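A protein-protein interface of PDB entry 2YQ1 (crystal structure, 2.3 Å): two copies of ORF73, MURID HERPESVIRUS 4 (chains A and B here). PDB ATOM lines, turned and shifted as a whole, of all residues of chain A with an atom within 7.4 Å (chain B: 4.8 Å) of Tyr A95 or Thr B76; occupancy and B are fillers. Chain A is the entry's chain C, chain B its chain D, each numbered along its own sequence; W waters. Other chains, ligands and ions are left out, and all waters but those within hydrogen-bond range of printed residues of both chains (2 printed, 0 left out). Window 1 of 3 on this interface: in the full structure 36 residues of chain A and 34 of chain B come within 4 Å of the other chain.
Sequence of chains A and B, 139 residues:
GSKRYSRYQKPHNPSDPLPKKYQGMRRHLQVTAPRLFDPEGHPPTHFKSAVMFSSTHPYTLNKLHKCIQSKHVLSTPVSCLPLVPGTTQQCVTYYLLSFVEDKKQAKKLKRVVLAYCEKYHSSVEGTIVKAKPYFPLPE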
ATOM      1  N   VAL A  51       9.507  -6.928  -5.462  1.00  0.00           N
ATOM      2  CA  VAL A  51      10.340  -6.205  -4.521  1.00  0.00           C
ATOM      3  C   VAL A  51      11.662  -6.942  -4.448  1.00  0.00           C
ATOM      4  O   VAL A  51      11.691  -8.147  -4.199  1.00  0.00           O
ATOM      5  CB  VAL A  51       9.734  -6.178  -3.104  1.00  0.00           C
ATOM      6  CG1 VAL A  51      10.644  -5.381  -2.163  1.00  0.00           C
ATOM      7  CG2 VAL A  51       8.333  -5.586  -3.122  1.00  0.00           C
ATOM      8  N   MET A  52      12.754  -6.229  -4.686  1.00  0.00           N
ATOM      9  CA  MET A  52      14.069  -6.790  -4.438  1.00  0.00           C
ATOM     10  C   MET A  52      14.457  -6.544  -2.990  1.00  0.00           C
ATOM     11  O   MET A  52      14.629  -5.402  -2.571  1.00  0.00           O
ATOM     12  CB  MET A  52      15.117  -6.185  -5.374  1.00  0.00           C
ATOM     13  CG  MET A  52      16.548  -6.596  -5.030  1.00  0.00           C
ATOM     14  SD  MET A  52      17.788  -5.838  -6.103  1.00  0.00           S
ATOM     15  CE  MET A  52      17.488  -6.712  -7.641  1.00  0.00           C
ATOM     16  N   PHE A  53      14.595  -7.621  -2.227  1.00  0.00           N
ATOM     17  CA  PHE A  53      15.084  -7.512  -0.859  1.00  0.00           C
ATOM     18  C   PHE A  53      16.578  -7.779  -0.826  1.00  0.00           C
ATOM     19  O   PHE A  53      17.041  -8.811  -1.299  1.00  0.00           O
ATOM     20  CB  PHE A  53      14.338  -8.481   0.055  1.00  0.00           C
ATOM     21  CG  PHE A  53      12.888  -8.143   0.229  1.00  0.00           C
ATOM     22  CD1 PHE A  53      12.502  -7.092   1.051  1.00  0.00           C
ATOM     23  CD2 PHE A  53      11.909  -8.853  -0.449  1.00  0.00           C
ATOM     24  CE1 PHE A  53      11.165  -6.769   1.203  1.00  0.00           C
ATOM     25  CE2 PHE A  53      10.572  -8.534  -0.299  1.00  0.00           C
ATOM     26  CZ  PHE A  53      10.199  -7.492   0.530  1.00  0.00           C
ATOM     27  N   SER A  54      17.331  -6.845  -0.262  1.00  0.00           N
ATOM     28  CA  SER A  54      18.784  -6.954  -0.250  1.00  0.00           C
ATOM     29  C   SER A  54      19.351  -6.759   1.144  1.00  0.00           C
ATOM     30  O   SER A  54      18.774  -6.053   1.968  1.00  0.00           O
ATOM     31  CB  SER A  54      19.406  -5.935  -1.210  1.00  0.00           C
ATOM     32  OG  SER A  54      18.913  -4.635  -0.948  1.00  0.00           O
ATOM     33  N   SER A  55      20.499  -7.380   1.386  1.00  0.00           N
ATOM     34  CA  SER A  55      21.154  -7.332   2.685  1.00  0.00           C
ATOM     35  C   SER A  55      22.606  -7.760   2.523  1.00  0.00           C
ATOM     36  O   SER A  55      22.917  -8.618   1.701  1.00  0.00           O
ATOM     37  CB  SER A  55      20.447  -8.264   3.670  1.00  0.00           C
ATOM     38  OG  SER A  55      21.221  -8.441   4.842  1.00  0.00           O
ATOM     39  N   THR A  56      23.495  -7.154   3.302  1.00  0.00           N
ATOM     40  CA  THR A  56      24.901  -7.540   3.290  1.00  0.00           C
ATOM     41  C   THR A  56      25.129  -8.805   4.113  1.00  0.00           C
ATOM     42  O   THR A  56      26.175  -9.445   4.008  1.00  0.00           O
ATOM     43  CB  THR A  56      25.800  -6.412   3.826  1.00  0.00           C
ATOM     44  OG1 THR A  56      25.378  -6.056   5.148  1.00  0.00           O
ATOM     45  CG2 THR A  56      25.708  -5.186   2.927  1.00  0.00           C
ATOM     46  N   HIS A  57      24.149  -9.161   4.937  1.00  0.00           N
ATOM     47  CA  HIS A  57      24.214 -10.406   5.692  1.00  0.00           C
ATOM     48  C   HIS A  57      23.903 -11.568   4.758  1.00  0.00           C
ATOM     49  O   HIS A  57      22.898 -11.542   4.049  1.00  0.00           O
ATOM     50  CB  HIS A  57      23.240 -10.372   6.869  1.00  0.00           C
ATOM     51  CG  HIS A  57      23.446 -11.478   7.856  1.00  0.00           C
ATOM     52  ND1 HIS A  57      23.252 -12.806   7.539  1.00  0.00           N
ATOM     53  CD2 HIS A  57      23.826 -11.454   9.155  1.00  0.00           C
ATOM     54  CE1 HIS A  57      23.509 -13.552   8.599  1.00  0.00           C
ATOM     55  NE2 HIS A  57      23.859 -12.756   9.593  1.00  0.00           N
ATOM     56  N   LEU A  61      18.481 -13.309   4.360  1.00  0.00           N
ATOM     57  CA  LEU A  61      17.522 -13.411   3.264  1.00  0.00           C
ATOM     58  C   LEU A  61      17.008 -14.839   3.039  1.00  0.00           C
ATOM     59  O   LEU A  61      16.049 -15.041   2.294  1.00  0.00           O
ATOM     60  CB  LEU A  61      18.109 -12.832   1.974  1.00  0.00           C
ATOM     61  CG  LEU A  61      18.541 -11.363   2.052  1.00  0.00           C
ATOM     62  CD1 LEU A  61      19.249 -10.960   0.778  1.00  0.00           C
ATOM     63  CD2 LEU A  61      17.365 -10.434   2.327  1.00  0.00           C
ATOM     64  N   THR A  76      12.520 -15.668  -5.464  1.00  0.00           N
ATOM     65  CA  THR A  76      13.722 -16.353  -5.912  1.00  0.00           C
ATOM     66  C   THR A  76      14.527 -16.820  -4.708  1.00  0.00           C
ATOM     67  O   THR A  76      14.364 -16.292  -3.606  1.00  0.00           O
ATOM     68  CB  THR A  76      14.623 -15.411  -6.743  1.00  0.00           C
ATOM     69  OG1 THR A  76      15.132 -14.373  -5.903  1.00  0.00           O
ATOM     70  CG2 THR A  76      13.855 -14.787  -7.895  1.00  0.00           C
ATOM     71  N   PRO A  77      15.411 -17.808  -4.911  1.00  0.00           N
ATOM     72  CA  PRO A  77      16.384 -18.063  -3.849  1.00  0.00           C
ATOM     73  C   PRO A  77      17.351 -16.892  -3.740  1.00  0.00           C
ATOM     74  O   PRO A  77      17.347 -15.989  -4.584  1.00  0.00           O
ATOM     75  CB  PRO A  77      17.123 -19.309  -4.345  1.00  0.00           C
ATOM     76  CG  PRO A  77      16.925 -19.319  -5.814  1.00  0.00           C
ATOM     77  CD  PRO A  77      15.563 -18.738  -6.043  1.00  0.00           C
ATOM     78  N   VAL A  78      18.196 -16.918  -2.720  1.00  0.00           N
ATOM     79  CA  VAL A  78      19.120 -15.822  -2.497  1.00  0.00           C
ATOM     80  C   VAL A  78      20.300 -15.889  -3.452  1.00  0.00           C
ATOM     81  O   VAL A  78      20.956 -16.919  -3.576  1.00  0.00           O
ATOM     82  CB  VAL A  78      19.639 -15.788  -1.049  1.00  0.00           C
ATOM     83  CG1 VAL A  78      20.375 -14.486  -0.794  1.00  0.00           C
ATOM     84  CG2 VAL A  78      18.492 -15.951  -0.064  1.00  0.00           C
ATOM     85  N   SER A  79      20.557 -14.782  -4.133  1.00  0.00           N
ATOM     86  CA  SER A  79      21.760 -14.647  -4.928  1.00  0.00           C
ATOM     87  C   SER A  79      22.516 -13.428  -4.419  1.00  0.00           C
ATOM     88  O   SER A  79      22.262 -12.938  -3.321  1.00  0.00           O
ATOM     89  CB  SER A  79      21.416 -14.492  -6.410  1.00  0.00           C
ATOM     90  OG  SER A  79      22.550 -14.710  -7.238  1.00  0.00           O
ATOM     91  N   CYS A  80      23.437 -12.926  -5.221  1.00  0.00           N
ATOM     92  CA  CYS A  80      24.220 -11.782  -4.804  1.00  0.00           C
ATOM     93  C   CYS A  80      24.330 -10.773  -5.935  1.00  0.00           C
ATOM     94  O   CYS A  80      24.277 -11.135  -7.113  1.00  0.00           O
ATOM     95  CB  CYS A  80      25.605 -12.233  -4.348  1.00  0.00           C
ATOM     96  SG  CYS A  80      26.629 -12.876  -5.667  1.00  0.00           S
ATOM     97  N   LEU A  81      24.458  -9.503  -5.567  1.00  0.00           N
ATOM     98  CA  LEU A  81      24.616  -8.435  -6.543  1.00  0.00           C
ATOM     99  C   LEU A  81      26.051  -8.421  -7.061  1.00  0.00           C
ATOM    100  O   LEU A  81      26.959  -8.907  -6.390  1.00  0.00           O
ATOM    101  CB  LEU A  81      24.252  -7.088  -5.911  1.00  0.00           C
ATOM    102  CG  LEU A  81      22.767  -6.905  -5.592  1.00  0.00           C
ATOM    103  CD1 LEU A  81      22.527  -5.618  -4.816  1.00  0.00           C
ATOM    104  CD2 LEU A  81      21.947  -6.929  -6.874  1.00  0.00           C
ATOM    105  N   PRO A  82      26.256  -7.885  -8.273  1.00  0.00           N
ATOM    106  CA  PRO A  82      27.616  -7.807  -8.821  1.00  0.00           C
ATOM    107  C   PRO A  82      28.456  -6.748  -8.116  1.00  0.00           C
ATOM    108  O   PRO A  82      27.918  -5.804  -7.539  1.00  0.00           O
ATOM    109  CB  PRO A  82      27.380  -7.402 -10.279  1.00  0.00           C
ATOM    110  CG  PRO A  82      26.060  -6.706 -10.263  1.00  0.00           C
ATOM    111  CD  PRO A  82      25.242  -7.411  -9.228  1.00  0.00           C
ATOM    112  N   LEU A  83      29.772  -6.904  -8.171  1.00  0.00           N
ATOM    113  CA  LEU A  83      30.666  -5.917  -7.584  1.00  0.00           C
ATOM    114  C   LEU A  83      30.775  -4.713  -8.509  1.00  0.00           C
ATOM    115  O   LEU A  83      30.744  -4.857  -9.733  1.00  0.00           O
ATOM    116  CB  LEU A  83      32.047  -6.522  -7.350  1.00  0.00           C
ATOM    117  CG  LEU A  83      32.112  -7.658  -6.328  1.00  0.00           C
ATOM    118  CD1 LEU A  83      33.444  -8.376  -6.418  1.00  0.00           C
ATOM    119  CD2 LEU A  83      31.878  -7.131  -4.920  1.00  0.00           C
ATOM    120  N   THR A  93      26.785  -7.764  -1.509  1.00  0.00           N
ATOM    121  CA  THR A  93      25.402  -7.542  -1.129  1.00  0.00           C
ATOM    122  C   THR A  93      24.558  -8.673  -1.704  1.00  0.00           C
ATOM    123  O   THR A  93      24.618  -8.964  -2.900  1.00  0.00           O
ATOM    124  CB  THR A  93      24.890  -6.181  -1.642  1.00  0.00           C
ATOM    125  OG1 THR A  93      25.718  -5.134  -1.119  1.00  0.00           O
ATOM    126  CG2 THR A  93      23.453  -5.943  -1.198  1.00  0.00           C
ATOM    127  N   TYR A  94      23.794  -9.329  -0.840  1.00  0.00           N
ATOM    128  CA  TYR A  94      22.949 -10.430  -1.270  1.00  0.00           C
ATOM    129  C   TYR A  94      21.549  -9.909  -1.566  1.00  0.00           C
ATOM    130  O   TYR A  94      21.158  -8.855  -1.068  1.00  0.00           O
ATOM    131  CB  TYR A  94      22.933 -11.536  -0.209  1.00  0.00           C
ATOM    132  CG  TYR A  94      24.316 -12.073   0.091  1.00  0.00           C
ATOM    133  CD1 TYR A  94      25.141 -11.445   1.019  1.00  0.00           C
ATOM    134  CD2 TYR A  94      24.808 -13.193  -0.570  1.00  0.00           C
ATOM    135  CE1 TYR A  94      26.409 -11.921   1.284  1.00  0.00           C
ATOM    136  CE2 TYR A  94      26.077 -13.679  -0.308  1.00  0.00           C
ATOM    137  CZ  TYR A  94      26.873 -13.041   0.619  1.00  0.00           C
ATOM    138  OH  TYR A  94      28.137 -13.520   0.882  1.00  0.00           O
ATOM    139  N   TYR A  95      20.791 -10.637  -2.376  1.00  0.00           N
ATOM    140  CA  TYR A  95      19.457 -10.174  -2.741  1.00  0.00           C
ATOM    141  C   TYR A  95      18.549 -11.327  -3.138  1.00  0.00           C
ATOM    142  O   TYR A  95      19.012 -12.417  -3.486  1.00  0.00           O
ATOM    143  CB  TYR A  95      19.521  -9.160  -3.892  1.00  0.00           C
ATOM    144  CG  TYR A  95      19.543  -9.826  -5.248  1.00  0.00           C
ATOM    145  CD1 TYR A  95      20.732 -10.285  -5.795  1.00  0.00           C
ATOM    146  CD2 TYR A  95      18.372 -10.000  -5.982  1.00  0.00           C
ATOM    147  CE1 TYR A  95      20.757 -10.907  -7.027  1.00  0.00           C
ATOM    148  CE2 TYR A  95      18.390 -10.622  -7.214  1.00  0.00           C
ATOM    149  CZ  TYR A  95      19.587 -11.069  -7.732  1.00  0.00           C
ATOM    150  OH  TYR A  95      19.612 -11.686  -8.960  1.00  0.00           O
ATOM    151  N   LEU A  96      17.249 -11.064  -3.113  1.00  0.00           N
ATOM    152  CA  LEU A  96      16.284 -11.941  -3.755  1.00  0.00           C
ATOM    153  C   LEU A  96      15.180 -11.096  -4.369  1.00  0.00           C
ATOM    154  O   LEU A  96      15.052  -9.912  -4.056  1.00  0.00           O
ATOM    155  CB  LEU A  96      15.725 -12.979  -2.769  1.00  0.00           C
ATOM    156  CG  LEU A  96      15.002 -12.556  -1.486  1.00  0.00           C
ATOM    157  CD1 LEU A  96      13.567 -12.088  -1.728  1.00  0.00           C
ATOM    158  CD2 LEU A  96      15.011 -13.714  -0.496  1.00  0.00           C
ATOM    159  N   LEU A  97      14.385 -11.704  -5.242  1.00  0.00           N
ATOM    160  CA  LEU A  97      13.259 -11.009  -5.843  1.00  0.00           C
ATOM    161  C   LEU A  97      11.968 -11.666  -5.386  1.00  0.00           C
ATOM    162  O   LEU A  97      11.809 -12.881  -5.484  1.00  0.00           O
ATOM    163  CB  LEU A  97      13.353 -11.070  -7.368  1.00  0.00           C
ATOM    164  CG  LEU A  97      14.592 -10.388  -7.944  1.00  0.00           C
ATOM    165  CD1 LEU A  97      14.724 -10.658  -9.432  1.00  0.00           C
ATOM    166  CD2 LEU A  97      14.510  -8.900  -7.672  1.00  0.00           C
ATOM    167  N   HIS B  65      26.635 -14.437 -18.195  1.00  0.00           N
ATOM    168  CA  HIS B  65      27.073 -13.855 -16.928  1.00  0.00           C
ATOM    169  C   HIS B  65      28.509 -13.358 -17.007  1.00  0.00           C
ATOM    170  O   HIS B  65      28.832 -12.293 -16.485  1.00  0.00           O
ATOM    171  CB  HIS B  65      26.925 -14.853 -15.774  1.00  0.00           C
ATOM    172  CG  HIS B  65      27.681 -14.462 -14.541  1.00  0.00           C
ATOM    173  ND1 HIS B  65      27.400 -13.319 -13.823  1.00  0.00           N
ATOM    174  CD2 HIS B  65      28.713 -15.061 -13.900  1.00  0.00           C
ATOM    175  CE1 HIS B  65      28.223 -13.233 -12.793  1.00  0.00           C
ATOM    176  NE2 HIS B  65      29.028 -14.279 -12.816  1.00  0.00           N
ATOM    177  N   LEU B  74      26.637  -4.378 -15.214  1.00  0.00           N
ATOM    178  CA  LEU B  74      26.974  -5.286 -14.129  1.00  0.00           C
ATOM    179  C   LEU B  74      25.937  -6.387 -14.036  1.00  0.00           C
ATOM    180  O   LEU B  74      24.779  -6.131 -13.713  1.00  0.00           O
ATOM    181  CB  LEU B  74      27.034  -4.522 -12.805  1.00  0.00           C
ATOM    182  CG  LEU B  74      27.831  -3.217 -12.742  1.00  0.00           C
ATOM    183  CD1 LEU B  74      27.838  -2.648 -11.333  1.00  0.00           C
ATOM    184  CD2 LEU B  74      29.244  -3.453 -13.206  1.00  0.00           C
ATOM    185  N   SER B  75      26.361  -7.613 -14.314  1.00  0.00           N
ATOM    186  CA  SER B  75      25.455  -8.753 -14.321  1.00  0.00           C
ATOM    187  C   SER B  75      25.651  -9.613 -13.083  1.00  0.00           C
ATOM    188  O   SER B  75      26.782  -9.919 -12.700  1.00  0.00           O
ATOM    189  CB  SER B  75      25.654  -9.595 -15.583  1.00  0.00           C
ATOM    190  OG  SER B  75      25.291  -8.880 -16.751  1.00  0.00           O
ATOM    191  N   THR B  76      24.545  -9.980 -12.449  1.00  0.00           N
ATOM    192  CA  THR B  76      24.554 -10.908 -11.326  1.00  0.00           C
ATOM    193  C   THR B  76      24.959 -12.294 -11.816  1.00  0.00           C
ATOM    194  O   THR B  76      24.902 -12.571 -13.013  1.00  0.00           O
ATOM    195  CB  THR B  76      23.135 -11.046 -10.741  1.00  0.00           C
ATOM    196  OG1 THR B  76      22.280 -11.653 -11.718  1.00  0.00           O
ATOM    197  CG2 THR B  76      22.573  -9.690 -10.359  1.00  0.00           C
ATOM    198  N   PRO B  77      25.389 -13.172 -10.895  1.00  0.00           N
ATOM    199  CA  PRO B  77      25.519 -14.585 -11.269  1.00  0.00           C
ATOM    200  C   PRO B  77      24.165 -15.181 -11.647  1.00  0.00           C
ATOM    201  O   PRO B  77      23.129 -14.536 -11.464  1.00  0.00           O
ATOM    202  CB  PRO B  77      26.050 -15.242  -9.989  1.00  0.00           C
ATOM    203  CG  PRO B  77      25.701 -14.290  -8.893  1.00  0.00           C
ATOM    204  CD  PRO B  77      25.813 -12.930  -9.507  1.00  0.00           C
ATOM    205  N   VAL B  78      24.173 -16.413 -12.141  1.00  0.00           N
ATOM    206  CA  VAL B  78      22.940 -17.074 -12.540  1.00  0.00           C
ATOM    207  C   VAL B  78      22.207 -17.640 -11.331  1.00  0.00           C
ATOM    208  O   VAL B  78      22.779 -18.375 -10.527  1.00  0.00           O
ATOM    209  CB  VAL B  78      23.209 -18.212 -13.548  1.00  0.00           C
ATOM    210  CG1 VAL B  78      21.903 -18.846 -13.998  1.00  0.00           C
ATOM    211  CG2 VAL B  78      23.988 -17.685 -14.749  1.00  0.00           C
ATOM    212  N   TYR B  95      17.912 -17.281 -14.609  1.00  0.00           N
ATOM    213  CA  TYR B  95      17.998 -15.874 -14.951  1.00  0.00           C
ATOM    214  C   TYR B  95      19.285 -15.249 -14.433  1.00  0.00           C
ATOM    215  O   TYR B  95      19.939 -15.778 -13.533  1.00  0.00           O
ATOM    216  CB  TYR B  95      16.803 -15.112 -14.375  1.00  0.00           C
ATOM    217  CG  TYR B  95      16.992 -14.673 -12.939  1.00  0.00           C
ATOM    218  CD1 TYR B  95      16.739 -15.546 -11.885  1.00  0.00           C
ATOM    219  CD2 TYR B  95      17.418 -13.384 -12.635  1.00  0.00           C
ATOM    220  CE1 TYR B  95      16.910 -15.151 -10.576  1.00  0.00           C
ATOM    221  CE2 TYR B  95      17.590 -12.980 -11.327  1.00  0.00           C
ATOM    222  CZ  TYR B  95      17.334 -13.867 -10.301  1.00  0.00           C
ATOM    223  OH  TYR B  95      17.503 -13.466  -8.997  1.00  0.00           O
ATOM    224  N   LEU B  96      19.631 -14.107 -15.014  1.00  0.00           N
ATOM    225  CA  LEU B  96      20.553 -13.178 -14.394  1.00  0.00           C
ATOM    226  C   LEU B  96      20.004 -11.782 -14.640  1.00  0.00           C
ATOM    227  O   LEU B  96      19.200 -11.579 -15.548  1.00  0.00           O
ATOM    228  CB  LEU B  96      21.967 -13.325 -14.965  1.00  0.00           C
ATOM    229  CG  LEU B  96      22.213 -12.945 -16.431  1.00  0.00           C
ATOM    230  CD1 LEU B  96      22.654 -11.499 -16.576  1.00  0.00           C
ATOM    231  CD2 LEU B  96      23.248 -13.870 -17.051  1.00  0.00           C
ATOM    232  N   LEU B  97      20.414 -10.824 -13.824  1.00  0.00           N
ATOM    233  CA  LEU B  97      20.086  -9.434 -14.088  1.00  0.00           C
ATOM    234  C   LEU B  97      21.333  -8.732 -14.584  1.00  0.00           C
ATOM    235  O   LEU B  97      22.402  -8.878 -13.996  1.00  0.00           O
ATOM    236  CB  LEU B  97      19.576  -8.745 -12.821  1.00  0.00           C
ATOM    237  CG  LEU B  97      18.139  -9.069 -12.409  1.00  0.00           C
ATOM    238  CD1 LEU B  97      17.858  -8.572 -10.994  1.00  0.00           C
ATOM    239  CD2 LEU B  97      17.140  -8.487 -13.405  1.00  0.00           C
ATOM    240  N   PHE B  99      22.575  -5.116 -14.833  1.00  0.00           N
ATOM    241  CA  PHE B  99      22.250  -3.756 -14.424  1.00  0.00           C
ATOM    242  C   PHE B  99      22.909  -2.715 -15.319  1.00  0.00           C
ATOM    243  O   PHE B  99      24.081  -2.832 -15.680  1.00  0.00           O
ATOM    244  CB  PHE B  99      22.623  -3.517 -12.963  1.00  0.00           C
ATOM    245  CG  PHE B  99      21.891  -4.407 -11.999  1.00  0.00           C
ATOM    246  CD1 PHE B  99      20.536  -4.229 -11.772  1.00  0.00           C
ATOM    247  CD2 PHE B  99      22.553  -5.418 -11.327  1.00  0.00           C
ATOM    248  CE1 PHE B  99      19.856  -5.041 -10.887  1.00  0.00           C
ATOM    249  CE2 PHE B  99      21.880  -6.232 -10.443  1.00  0.00           C
ATOM    250  CZ  PHE B  99      20.526  -6.046 -10.223  1.00  0.00           C
HETATM  251  O   HOH W   1      21.802 -13.882  -9.538  1.00  0.00           O
HETATM  252  O   HOH W   2      18.324 -14.680  -6.897  1.00  0.00           O
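OH of Tyr A95 sits at hydrogen-bond distance from OH of Tyr B95 (2.8 Å).
OG1 of Thr A76 is in hydrogen-bond range of N of Leu A97.
O of Ser A79 sits at hydrogen-bond distance from N of Tyr A95 (2.9 Å).
The backbone NH of Leu A81 is in hydrogen-bond range of the backbone carbonyl oxygen of Thr A93, at 2.7 Å.
O of Thr B76 is in hydrogen-bond range of ND1 of His B65 (2.7 Å).
The backbone carbonyl oxygen (O) of Leu B74 is in hydrogen-bond range of the backbone NH (N) of Phe B99, 2.7 Å away.
The backbone NH (N) of Thr B76 sits at hydrogen-bond distance from the backbone carbonyl oxygen (O) of Leu B97, 2.9 Å away.
Ser A79 touches Pro B77.
Cys A80 touches Thr B76.
Cys A80 touches Pro B77.
Leu A81 touches Phe B99 (CD2 to CE2, 3.6 Å).
CG of Pro A82 touches CB of Leu B74, at 3.5 Å.
Ser B75 touches Pro A82.
Pro A82 touches Thr B76.
Leu B74 touches Leu A83.
CG2 of Thr B76 touches OH of Tyr A95 (3.8 Å).
Tyr B95 touches Leu A97.
Printed residues of chain B within 4 Å of Leu A81: Phe B99.
Of chain B, only Thr B76 (3.8 Å) and Tyr B95 (2.8 Å) come within 4 Å of Tyr A95.
Of the printed residues of chain A, Leu B74 touches Pro A82 (3.5 Å) and Leu A83 (3.99 Å).
Thr B76 touches just these residues of chain A: Cys A80 (3.8 Å), Pro A82 (3.7 Å) and Tyr A95 (3.8 Å).
Hydrophobic or aromatic side chains of chain B that line the printed part of chain A: Leu B74, Pro B77, Tyr B95, Leu B97 and Phe B99.
Printed residues of chain A that touch a printed residue of chain B: Met A52, Ser A79, Cys A80, Leu A81, Pro A82, Leu A83, Tyr A95 and Leu A97.
Hydrophobic or aromatic side chains of chain A that line the printed part of chain B: Met A52, Leu A81, Pro A82, Tyr A95 and Leu A97.
Along chain A the printed residues that touch a printed residue of chain B span positions 52 to 97.
Among the printed residues, 13 pairs touch across the chains.
Among the printed residues, no Asp or Glu carboxylate lies within 4 Å of a Lys or Arg side-chain nitrogen of the other chain.
Tyr A95 touches Thr B76, but with the chains exchanged Thr A76 does not touch Tyr B95 (4.002 Å).
Tyr B95 touches its own counterpart, Tyr A95.
Leu A97 touches Tyr B95, but with the chains exchanged Tyr A95 does not touch Leu B97 (4.1 Å).
Water W1 lies within hydrogen-bond range of O of Pro B77 (2.4 Å), OG of Ser A79 (2.6 Å), OG1 of Thr B76 (3.2 Å) and OH of Tyr A95 (3.2 Å).
Water W2 lies within hydrogen-bond range of the side-chain hydroxyl (OH) of Tyr B95 (2.6 Å), the backbone carbonyl oxygen (O) of Pro A77 (2.8 Å) and the side-chain hydroxyl (OG1) of Thr A76 (3.4 Å).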
